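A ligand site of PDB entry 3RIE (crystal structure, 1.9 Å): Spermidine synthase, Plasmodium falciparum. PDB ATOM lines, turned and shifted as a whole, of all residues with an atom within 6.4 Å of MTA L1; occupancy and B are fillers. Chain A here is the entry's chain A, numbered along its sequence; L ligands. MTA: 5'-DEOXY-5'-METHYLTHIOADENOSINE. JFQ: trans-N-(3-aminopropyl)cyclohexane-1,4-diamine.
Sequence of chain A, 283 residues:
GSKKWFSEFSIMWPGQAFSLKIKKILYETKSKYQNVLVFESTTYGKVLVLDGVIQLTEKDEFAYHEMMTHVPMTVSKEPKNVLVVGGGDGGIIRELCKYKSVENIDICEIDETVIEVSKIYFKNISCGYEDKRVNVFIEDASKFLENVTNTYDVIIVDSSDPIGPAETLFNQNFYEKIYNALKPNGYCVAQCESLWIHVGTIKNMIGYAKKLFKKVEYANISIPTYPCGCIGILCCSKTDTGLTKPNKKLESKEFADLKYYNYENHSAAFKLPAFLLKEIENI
N of Glu 139 sits at hydrogen-bond distance from O of Glu 109.
The side-chain carboxylate (OE1) of Glu 109 is in hydrogen-bond range of the backbone NH (N) of Gly 88, at 2.9 Å.
OD1 of Asp 140 is in hydrogen-bond range of N of Ser 142, at 2.9 Å.
OD2 of Asp 111 is in hydrogen-bond range of NE2 of Gln 34 (2.7 Å).
The backbone NH (N) of Gly 87 is in hydrogen-bond range of the backbone carbonyl oxygen (O) of Asp 158 (2.9 Å).
The backbone NH (N) of Asp 158 is in hydrogen-bond range of the backbone carbonyl oxygen (O) of Val 85 (2.8 Å).
The backbone carbonyl oxygen (O) of Glu 139 sits at hydrogen-bond distance from the side-chain sulfur (SG) of Cys 108 (3.2 Å).
The backbone NH of Gln 55 is in hydrogen-bond range of the backbone carbonyl oxygen of Leu 48, at 2.7 Å.
A sulfur (S5') of MTA L1 sits close to a nitrogen (N1) of JFQ L2.
The side-chain carboxylate (OD2) of Asp 89 sits close to a sulfur (S5') of MTA L1, 3.2 Å away.
Residues that only touch MTA L1: Leu 50, Gln 55, Gly 86, Gly 88, Cys 108, Asp 111, Val 114, Glu 139, Asp 158, Ser 159, Thr 168 and Leu 169.
Hydrophobic or aromatic side chains that line MTA L1: Leu 50, Ile 110, Val 114, Ala 141, Pro 165, Ala 166 and Leu 169.
Of the 31 residues printed, 22 come within 4 Å of MTA L1.
The side-chain carboxylate (OE2) of Glu 109 lies within hydrogen-bond range of an oxygen (O2') of MTA L1.
The side-chain carboxylate (OD1) of Asp 140 is in hydrogen-bond range of a nitrogen (N6) of MTA L1 (2.9 Å).
N of Ala 141 is in hydrogen-bond range of N1 of MTA L1, 2.9 Å away.
O of Pro 165 lies within hydrogen-bond range of N6 of MTA L1 (3.2 Å).
N7 of MTA L1 lies within hydrogen-bond range of N of Ala 166, at 3.2 Å.
A nitrogen (N3) of MTA L1 sits at hydrogen-bond distance from the backbone NH (N) of Ile 110 (3.2 Å).
The backbone NH of Ser 160 lies close to an oxygen (O4') of MTA L1, 3.5 Å away.
An oxygen (O2') of MTA L1 lies within hydrogen-bond range of the side-chain amide nitrogen (NE2) of Gln 34, at 3.3 Å.
N of Gly 87 lies close to S5' of MTA L1.
The side-chain carboxylate (OD2) of Asp 89 lies within salt-bridge range of a nitrogen (N1) of JFQ L2.
The side-chain carboxylate of Asp 158 lies within salt-bridge range of a nitrogen (N1) of JFQ L2, 2.9 Å away.
The backbone carbonyl oxygen of Ser 159 lies within hydrogen-bond range of a nitrogen (N2) of JFQ L2, 3.0 Å away.
The side-chain carboxylate (OD2) of Asp 161 is in salt-bridge range of a nitrogen (N3) of JFQ L2.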
ATOM      1  N   TYR A  33      19.476 -19.451   4.883  1.00  0.00           N
ATOM      2  CA  TYR A  33      18.708 -20.681   5.138  1.00  0.00           C
ATOM      3  C   TYR A  33      18.350 -20.970   6.569  1.00  0.00           C
ATOM      4  O   TYR A  33      17.358 -21.629   6.798  1.00  0.00           O
ATOM      5  CB  TYR A  33      19.379 -21.928   4.518  1.00  0.00           C
ATOM      6  CG  TYR A  33      19.530 -21.812   3.014  1.00  0.00           C
ATOM      7  CD1 TYR A  33      18.471 -22.145   2.148  1.00  0.00           C
ATOM      8  CD2 TYR A  33      20.711 -21.354   2.460  1.00  0.00           C
ATOM      9  CE1 TYR A  33      18.595 -22.027   0.778  1.00  0.00           C
ATOM     10  CE2 TYR A  33      20.871 -21.248   1.124  1.00  0.00           C
ATOM     11  CZ  TYR A  33      19.825 -21.587   0.286  1.00  0.00           C
ATOM     12  OH  TYR A  33      20.013 -21.471  -1.018  1.00  0.00           O
ATOM     13  N   GLN A  34      19.167 -20.530   7.516  1.00  0.00           N
ATOM     14  CA  GLN A  34      19.057 -21.075   8.863  1.00  0.00           C
ATOM     15  C   GLN A  34      19.544 -20.042   9.818  1.00  0.00           C
ATOM     16  O   GLN A  34      20.344 -19.145   9.444  1.00  0.00           O
ATOM     17  CB  GLN A  34      20.018 -22.272   9.033  1.00  0.00           C
ATOM     18  CG  GLN A  34      19.876 -23.274   8.048  1.00  0.00           C
ATOM     19  CD  GLN A  34      21.024 -24.279   8.009  1.00  0.00           C
ATOM     20  OE1 GLN A  34      20.962 -25.386   8.620  1.00  0.00           O
ATOM     21  NE2 GLN A  34      22.102 -23.832   7.463  1.00  0.00           N
ATOM     22  N   LEU A  48      28.402 -25.869  17.406  1.00  0.00           N
ATOM     23  CA  LEU A  48      27.707 -25.299  16.266  1.00  0.00           C
ATOM     24  C   LEU A  48      26.237 -25.702  16.328  1.00  0.00           C
ATOM     25  O   LEU A  48      25.909 -26.892  16.489  1.00  0.00           O
ATOM     26  CB  LEU A  48      28.358 -25.758  14.935  1.00  0.00           C
ATOM     27  CG  LEU A  48      27.466 -25.440  13.702  1.00  0.00           C
ATOM     28  CD1 LEU A  48      27.520 -23.918  13.421  1.00  0.00           C
ATOM     29  CD2 LEU A  48      28.036 -26.103  12.465  1.00  0.00           C
ATOM     30  N   LEU A  50      22.421 -25.033  14.439  1.00  0.00           N
ATOM     31  CA  LEU A  50      21.656 -24.533  13.314  1.00  0.00           C
ATOM     32  C   LEU A  50      20.160 -24.678  13.617  1.00  0.00           C
ATOM     33  O   LEU A  50      19.718 -25.759  13.930  1.00  0.00           O
ATOM     34  CB  LEU A  50      22.009 -25.267  12.002  1.00  0.00           C
ATOM     35  CG  LEU A  50      23.466 -25.228  11.555  1.00  0.00           C
ATOM     36  CD1 LEU A  50      23.686 -26.143  10.289  1.00  0.00           C
ATOM     37  CD2 LEU A  50      23.839 -23.770  11.275  1.00  0.00           C
ATOM     38  N   GLN A  55      24.605 -29.212  16.010  1.00  0.00           N
ATOM     39  CA  GLN A  55      25.197 -29.961  14.857  1.00  0.00           C
ATOM     40  C   GLN A  55      26.473 -30.682  15.318  1.00  0.00           C
ATOM     41  O   GLN A  55      26.728 -31.801  14.939  1.00  0.00           O
ATOM     42  CB  GLN A  55      25.527 -29.015  13.666  1.00  0.00           C
ATOM     43  CG  GLN A  55      24.366 -28.234  13.234  1.00  0.00           C
ATOM     44  CD  GLN A  55      23.262 -29.082  12.652  1.00  0.00           C
ATOM     45  OE1 GLN A  55      23.512 -29.833  11.713  1.00  0.00           O
ATOM     46  NE2 GLN A  55      21.993 -28.957  13.201  1.00  0.00           N
ATOM     47  N   LEU A  56      27.277 -30.041  16.139  1.00  0.00           N
ATOM     48  CA  LEU A  56      28.463 -30.699  16.583  1.00  0.00           C
ATOM     49  C   LEU A  56      28.952 -29.950  17.763  1.00  0.00           C
ATOM     50  O   LEU A  56      28.585 -28.781  17.971  1.00  0.00           O
ATOM     51  CB  LEU A  56      29.570 -30.760  15.507  1.00  0.00           C
ATOM     52  CG  LEU A  56      30.139 -29.483  14.811  1.00  0.00           C
ATOM     53  CD1 LEU A  56      31.202 -28.898  15.665  1.00  0.00           C
ATOM     54  CD2 LEU A  56      30.831 -29.934  13.446  1.00  0.00           C
ATOM     55  N   VAL A  85      27.060 -34.957   1.034  1.00  0.00           N
ATOM     56  CA  VAL A  85      25.840 -34.141   0.978  1.00  0.00           C
ATOM     57  C   VAL A  85      25.703 -33.438   2.359  1.00  0.00           C
ATOM     58  O   VAL A  85      25.864 -34.096   3.446  1.00  0.00           O
ATOM     59  CB  VAL A  85      24.611 -34.961   0.562  1.00  0.00           C
ATOM     60  CG1 VAL A  85      23.283 -34.163   0.738  1.00  0.00           C
ATOM     61  CG2 VAL A  85      24.754 -35.515  -0.914  1.00  0.00           C
ATOM     62  N   GLY A  86      25.533 -32.099   2.338  1.00  0.00           N
ATOM     63  CA  GLY A  86      25.485 -31.367   3.600  1.00  0.00           C
ATOM     64  C   GLY A  86      26.908 -31.314   4.090  1.00  0.00           C
ATOM     65  O   GLY A  86      27.843 -31.029   3.317  1.00  0.00           O
ATOM     66  N   GLY A  87      27.120 -31.506   5.368  1.00  0.00           N
ATOM     67  CA  GLY A  87      28.520 -31.559   5.917  1.00  0.00           C
ATOM     68  C   GLY A  87      29.400 -30.325   5.844  1.00  0.00           C
ATOM     69  O   GLY A  87      30.682 -30.425   5.927  1.00  0.00           O
ATOM     70  N   GLY A  88      28.766 -29.142   5.757  1.00  0.00           N
ATOM     71  CA  GLY A  88      29.489 -27.864   5.645  1.00  0.00           C
ATOM     72  C   GLY A  88      30.599 -27.693   6.637  1.00  0.00           C
ATOM     73  O   GLY A  88      31.585 -27.017   6.362  1.00  0.00           O
ATOM     74  N   ASP A  89      30.471 -28.289   7.838  1.00  0.00           N
ATOM     75  CA  ASP A  89      31.506 -28.094   8.838  1.00  0.00           C
ATOM     76  C   ASP A  89      32.840 -28.704   8.420  1.00  0.00           C
ATOM     77  O   ASP A  89      33.902 -28.354   8.948  1.00  0.00           O
ATOM     78  CB  ASP A  89      31.061 -28.720  10.206  1.00  0.00           C
ATOM     79  CG  ASP A  89      30.639 -30.183  10.039  1.00  0.00           C
ATOM     80  OD1 ASP A  89      31.534 -31.074  10.032  1.00  0.00           O
ATOM     81  OD2 ASP A  89      29.440 -30.378   9.802  1.00  0.00           O
ATOM     82  N   CYS A 108      28.487 -31.009  -1.653  1.00  0.00           N
ATOM     83  CA  CYS A 108      27.384 -30.172  -1.942  1.00  0.00           C
ATOM     84  C   CYS A 108      26.691 -29.714  -0.649  1.00  0.00           C
ATOM     85  O   CYS A 108      25.949 -30.510  -0.019  1.00  0.00           O
ATOM     86  CB  CYS A 108      26.435 -30.955  -2.820  1.00  0.00           C
ATOM     87  SG  CYS A 108      25.102 -29.960  -3.322  1.00  0.00           S
ATOM     88  N   GLU A 109      26.947 -28.442  -0.286  1.00  0.00           N
ATOM     89  CA  GLU A 109      26.433 -27.862   0.955  1.00  0.00           C
ATOM     90  C   GLU A 109      25.616 -26.629   0.544  1.00  0.00           C
ATOM     91  O   GLU A 109      26.080 -25.777  -0.246  1.00  0.00           O
ATOM     92  CB  GLU A 109      27.605 -27.495   1.906  1.00  0.00           C
ATOM     93  CG  GLU A 109      27.213 -26.317   2.799  1.00  0.00           C
ATOM     94  CD  GLU A 109      26.226 -26.735   3.883  1.00  0.00           C
ATOM     95  OE1 GLU A 109      26.576 -27.651   4.699  1.00  0.00           O
ATOM     96  OE2 GLU A 109      25.151 -26.172   3.907  1.00  0.00           O
ATOM     97  N   ILE A 110      24.392 -26.557   1.046  1.00  0.00           N
ATOM     98  CA  ILE A 110      23.444 -25.547   0.480  1.00  0.00           C
ATOM     99  C   ILE A 110      23.808 -24.158   1.057  1.00  0.00           C
ATOM    100  O   ILE A 110      23.602 -23.108   0.425  1.00  0.00           O
ATOM    101  CB  ILE A 110      21.998 -25.896   0.818  1.00  0.00           C
ATOM    102  CG1 ILE A 110      21.002 -24.968   0.098  1.00  0.00           C
ATOM    103  CG2 ILE A 110      21.765 -25.847   2.426  1.00  0.00           C
ATOM    104  CD1 ILE A 110      19.505 -25.489   0.162  1.00  0.00           C
ATOM    105  N   ASP A 111      24.424 -24.167   2.226  1.00  0.00           N
ATOM    106  CA  ASP A 111      24.599 -22.913   3.013  1.00  0.00           C
ATOM    107  C   ASP A 111      26.098 -22.520   3.169  1.00  0.00           C
ATOM    108  O   ASP A 111      26.778 -23.082   4.002  1.00  0.00           O
ATOM    109  CB  ASP A 111      23.904 -23.064   4.387  1.00  0.00           C
ATOM    110  CG  ASP A 111      23.769 -21.708   5.122  1.00  0.00           C
ATOM    111  OD1 ASP A 111      24.463 -20.710   4.735  1.00  0.00           O
ATOM    112  OD2 ASP A 111      22.976 -21.667   6.064  1.00  0.00           O
ATOM    113  N   VAL A 114      27.787 -21.806   6.534  1.00  0.00           N
ATOM    114  CA  VAL A 114      28.216 -22.894   7.447  1.00  0.00           C
ATOM    115  C   VAL A 114      29.692 -23.199   7.137  1.00  0.00           C
ATOM    116  O   VAL A 114      30.502 -23.296   8.077  1.00  0.00           O
ATOM    117  CB  VAL A 114      27.332 -24.210   7.327  1.00  0.00           C
ATOM    118  CG1 VAL A 114      27.977 -25.367   8.123  1.00  0.00           C
ATOM    119  CG2 VAL A 114      25.850 -23.928   7.791  1.00  0.00           C
ATOM    120  N   ILE A 115      30.056 -23.330   5.848  1.00  0.00           N
ATOM    121  CA  ILE A 115      31.468 -23.557   5.511  1.00  0.00           C
ATOM    122  C   ILE A 115      32.371 -22.428   6.085  1.00  0.00           C
ATOM    123  O   ILE A 115      33.436 -22.698   6.701  1.00  0.00           O
ATOM    124  CB  ILE A 115      31.664 -23.710   3.998  1.00  0.00           C
ATOM    125  CG1 ILE A 115      30.868 -24.922   3.508  1.00  0.00           C
ATOM    126  CG2 ILE A 115      33.159 -23.820   3.609  1.00  0.00           C
ATOM    127  CD1 ILE A 115      30.980 -25.106   1.983  1.00  0.00           C
ATOM    128  N   GLU A 139      24.944 -25.468  -3.271  1.00  0.00           N
ATOM    129  CA  GLU A 139      23.605 -25.669  -3.795  1.00  0.00           C
ATOM    130  C   GLU A 139      22.830 -26.760  -3.056  1.00  0.00           C
ATOM    131  O   GLU A 139      23.391 -27.499  -2.308  1.00  0.00           O
ATOM    132  CB  GLU A 139      23.625 -25.918  -5.312  1.00  0.00           C
ATOM    133  CG  GLU A 139      24.440 -27.054  -5.779  1.00  0.00           C
ATOM    134  CD  GLU A 139      24.427 -27.275  -7.314  1.00  0.00           C
ATOM    135  OE1 GLU A 139      23.403 -27.556  -7.885  1.00  0.00           O
ATOM    136  OE2 GLU A 139      25.466 -27.204  -7.922  1.00  0.00           O
ATOM    137  N   ASP A 140      21.535 -26.804  -3.278  1.00  0.00           N
ATOM    138  CA  ASP A 140      20.681 -27.750  -2.626  1.00  0.00           C
ATOM    139  C   ASP A 140      21.086 -29.142  -3.203  1.00  0.00           C
ATOM    140  O   ASP A 140      21.086 -29.313  -4.430  1.00  0.00           O
ATOM    141  CB  ASP A 140      19.225 -27.414  -2.996  1.00  0.00           C
ATOM    142  CG  ASP A 140      18.180 -28.298  -2.243  1.00  0.00           C
ATOM    143  OD1 ASP A 140      18.449 -29.457  -1.865  1.00  0.00           O
ATOM    144  OD2 ASP A 140      17.033 -27.864  -2.044  1.00  0.00           O
ATOM    145  N   ALA A 141      21.404 -30.114  -2.340  1.00  0.00           N
ATOM    146  CA  ALA A 141      21.781 -31.443  -2.847  1.00  0.00           C
ATOM    147  C   ALA A 141      20.673 -32.106  -3.671  1.00  0.00           C
ATOM    148  O   ALA A 141      20.942 -32.932  -4.554  1.00  0.00           O
ATOM    149  CB  ALA A 141      22.258 -32.350  -1.710  1.00  0.00           C
ATOM    150  N   SER A 142      19.435 -31.718  -3.402  1.00  0.00           N
ATOM    151  CA  SER A 142      18.330 -32.262  -4.149  1.00  0.00           C
ATOM    152  C   SER A 142      18.468 -31.904  -5.656  1.00  0.00           C
ATOM    153  O   SER A 142      18.222 -32.768  -6.523  1.00  0.00           O
ATOM    154  CB  SER A 142      16.981 -31.789  -3.534  1.00  0.00           C
ATOM    155  OG  SER A 142      15.953 -32.005  -4.478  1.00  0.00           O
ATOM    156  N   ASP A 158      25.358 -36.260   5.123  1.00  0.00           N
ATOM    157  CA  ASP A 158      25.534 -35.652   6.407  1.00  0.00           C
ATOM    158  C   ASP A 158      24.661 -34.398   6.463  1.00  0.00           C
ATOM    159  O   ASP A 158      25.153 -33.330   6.472  1.00  0.00           O
ATOM    160  CB  ASP A 158      26.995 -35.325   6.597  1.00  0.00           C
ATOM    161  CG  ASP A 158      27.308 -34.687   7.919  1.00  0.00           C
ATOM    162  OD1 ASP A 158      26.554 -34.791   8.856  1.00  0.00           O
ATOM    163  OD2 ASP A 158      28.336 -34.087   7.997  1.00  0.00           O
ATOM    164  N   SER A 159      23.347 -34.624   6.508  1.00  0.00           N
ATOM    165  CA  SER A 159      22.379 -33.532   6.546  1.00  0.00           C
ATOM    166  C   SER A 159      22.040 -33.133   7.999  1.00  0.00           C
ATOM    167  O   SER A 159      22.202 -33.915   8.942  1.00  0.00           O
ATOM    168  CB  SER A 159      21.058 -33.953   5.873  1.00  0.00           C
ATOM    169  OG  SER A 159      20.569 -35.085   6.636  1.00  0.00           O
ATOM    170  N   SER A 160      21.650 -31.879   8.177  1.00  0.00           N
ATOM    171  CA  SER A 160      20.844 -31.452   9.322  1.00  0.00           C
ATOM    172  C   SER A 160      19.415 -32.155   9.276  1.00  0.00           C
ATOM    173  O   SER A 160      19.109 -32.947   8.347  1.00  0.00           O
ATOM    174  CB  SER A 160      20.707 -29.927   9.281  1.00  0.00           C
ATOM    175  OG  SER A 160      20.176 -29.514   8.017  1.00  0.00           O
ATOM    176  N   ASP A 161      18.554 -31.843  10.255  1.00  0.00           N
ATOM    177  CA  ASP A 161      17.229 -32.500  10.396  1.00  0.00           C
ATOM    178  C   ASP A 161      16.144 -32.071   9.391  1.00  0.00           C
ATOM    179  O   ASP A 161      16.283 -31.038   8.677  1.00  0.00           O
ATOM    180  CB  ASP A 161      16.727 -32.283  11.865  1.00  0.00           C
ATOM    181  CG  ASP A 161      17.560 -32.994  12.870  1.00  0.00           C
ATOM    182  OD1 ASP A 161      17.715 -34.227  12.686  1.00  0.00           O
ATOM    183  OD2 ASP A 161      18.042 -32.372  13.853  1.00  0.00           O
ATOM    184  N   GLY A 164      13.705 -27.469   8.001  1.00  0.00           N
ATOM    185  CA  GLY A 164      14.651 -26.519   7.458  1.00  0.00           C
ATOM    186  C   GLY A 164      15.117 -26.944   6.055  1.00  0.00           C
ATOM    187  O   GLY A 164      14.367 -27.617   5.334  1.00  0.00           O
ATOM    188  N   PRO A 165      16.339 -26.542   5.646  1.00  0.00           N
ATOM    189  CA  PRO A 165      16.605 -26.816   4.186  1.00  0.00           C
ATOM    190  C   PRO A 165      16.834 -28.306   3.938  1.00  0.00           C
ATOM    191  O   PRO A 165      16.827 -28.730   2.799  1.00  0.00           O
ATOM    192  CB  PRO A 165      17.859 -26.004   3.885  1.00  0.00           C
ATOM    193  CG  PRO A 165      18.572 -25.920   5.260  1.00  0.00           C
ATOM    194  CD  PRO A 165      17.436 -25.785   6.270  1.00  0.00           C
ATOM    195  N   ALA A 166      17.025 -29.113   4.965  1.00  0.00           N
ATOM    196  CA  ALA A 166      17.192 -30.558   4.742  1.00  0.00           C
ATOM    197  C   ALA A 166      15.889 -31.288   4.477  1.00  0.00           C
ATOM    198  O   ALA A 166      15.875 -32.508   4.340  1.00  0.00           O
ATOM    199  CB  ALA A 166      17.929 -31.198   5.840  1.00  0.00           C
ATOM    200  N   GLU A 167      14.792 -30.534   4.414  1.00  0.00           N
ATOM    201  CA  GLU A 167      13.460 -31.177   4.272  1.00  0.00           C
ATOM    202  C   GLU A 167      13.346 -31.988   2.978  1.00  0.00           C
ATOM    203  O   GLU A 167      12.641 -32.981   2.937  1.00  0.00           O
ATOM    204  CB  GLU A 167      12.335 -30.156   4.378  1.00  0.00           C
ATOM    205  CG  GLU A 167      12.321 -29.116   3.277  1.00  0.00           C
ATOM    206  CD  GLU A 167      11.371 -27.957   3.586  1.00  0.00           C
ATOM    207  OE1 GLU A 167      10.217 -28.238   4.053  1.00  0.00           O
ATOM    208  OE2 GLU A 167      11.795 -26.786   3.373  1.00  0.00           O
ATOM    209  N   THR A 168      14.097 -31.578   1.952  1.00  0.00           N
ATOM    210  CA  THR A 168      14.186 -32.308   0.697  1.00  0.00           C
ATOM    211  C   THR A 168      15.050 -33.597   0.715  1.00  0.00           C
ATOM    212  O   THR A 168      15.097 -34.295  -0.276  1.00  0.00           O
ATOM    213  CB  THR A 168      14.705 -31.378  -0.437  1.00  0.00           C
ATOM    214  OG1 THR A 168      16.034 -30.952  -0.118  1.00  0.00           O
ATOM    215  CG2 THR A 168      13.877 -30.144  -0.534  1.00  0.00           C
ATOM    216  N   LEU A 169      15.748 -33.930   1.794  1.00  0.00           N
ATOM    217  CA  LEU A 169      16.639 -35.096   1.716  1.00  0.00           C
ATOM    218  C   LEU A 169      16.024 -36.386   2.370  1.00  0.00           C
ATOM    219  O   LEU A 169      16.721 -37.421   2.634  1.00  0.00           O
ATOM    220  CB  LEU A 169      18.015 -34.695   2.246  1.00  0.00           C
ATOM    221  CG  LEU A 169      18.627 -33.356   1.772  1.00  0.00           C
ATOM    222  CD1 LEU A 169      19.958 -33.227   2.485  1.00  0.00           C
ATOM    223  CD2 LEU A 169      18.844 -33.323   0.283  1.00  0.00           C
HETATM  224  CS  MTA L   1      26.465 -28.893   9.721  1.00  0.00           C
HETATM  225  S5' MTA L   1      26.436 -30.353   8.688  1.00  0.00           S
HETATM  226  C5' MTA L   1      24.775 -30.443   7.999  1.00  0.00           C
HETATM  227  C4' MTA L   1      24.664 -29.477   6.839  1.00  0.00           C
HETATM  228  O4' MTA L   1      23.572 -29.921   6.064  1.00  0.00           O
HETATM  229  C2' MTA L   1      23.134 -27.709   6.277  1.00  0.00           C
HETATM  230  O2' MTA L   1      23.103 -26.401   5.678  1.00  0.00           O
HETATM  231  C3' MTA L   1      24.253 -28.057   7.234  1.00  0.00           C
HETATM  232  O3' MTA L   1      25.407 -27.277   7.127  1.00  0.00           O
HETATM  233  C1' MTA L   1      23.379 -28.782   5.238  1.00  0.00           C
HETATM  234  N9  MTA L   1      22.185 -28.973   4.453  1.00  0.00           N
HETATM  235  C8  MTA L   1      20.914 -28.941   4.892  1.00  0.00           C
HETATM  236  N7  MTA L   1      20.017 -29.075   3.887  1.00  0.00           N
HETATM  237  C5  MTA L   1      20.789 -29.319   2.773  1.00  0.00           C
HETATM  238  C6  MTA L   1      20.530 -29.556   1.359  1.00  0.00           C
HETATM  239  N6  MTA L   1      19.238 -29.617   0.937  1.00  0.00           N
HETATM  240  N1  MTA L   1      21.603 -29.656   0.532  1.00  0.00           N
HETATM  241  C2  MTA L   1      22.871 -29.510   0.925  1.00  0.00           C
HETATM  242  N3  MTA L   1      23.185 -29.319   2.228  1.00  0.00           N
HETATM  243  C4  MTA L   1      22.206 -29.216   3.142  1.00  0.00           C
HETATM  244  C1  JFQ L   2      27.743 -32.644  11.846  1.00  0.00           C
HETATM  245  N1  JFQ L   2      28.527 -32.769  10.549  1.00  0.00           N
HETATM  246  C2  JFQ L   2      26.267 -32.395  11.499  1.00  0.00           C
HETATM  247  N2  JFQ L   2      24.194 -33.666  11.136  1.00  0.00           N
HETATM  248  C3  JFQ L   2      25.489 -33.683  11.797  1.00  0.00           C
HETATM  249  N3  JFQ L   2      20.107 -33.831  15.391  1.00  0.00           N
HETATM  250  C4  JFQ L   2      23.036 -33.737  12.114  1.00  0.00           C
HETATM  251  C5  JFQ L   2      22.977 -32.590  13.136  1.00  0.00           C
HETATM  252  C6  JFQ L   2      21.574 -32.593  13.772  1.00  0.00           C
HETATM  253  C7  JFQ L   2      21.406 -33.856  14.639  1.00  0.00           C
HETATM  254  C8  JFQ L   2      21.555 -35.102  13.772  1.00  0.00           C
HETATM  255  C9  JFQ L   2      22.801 -35.089  12.826  1.00  0.00           C
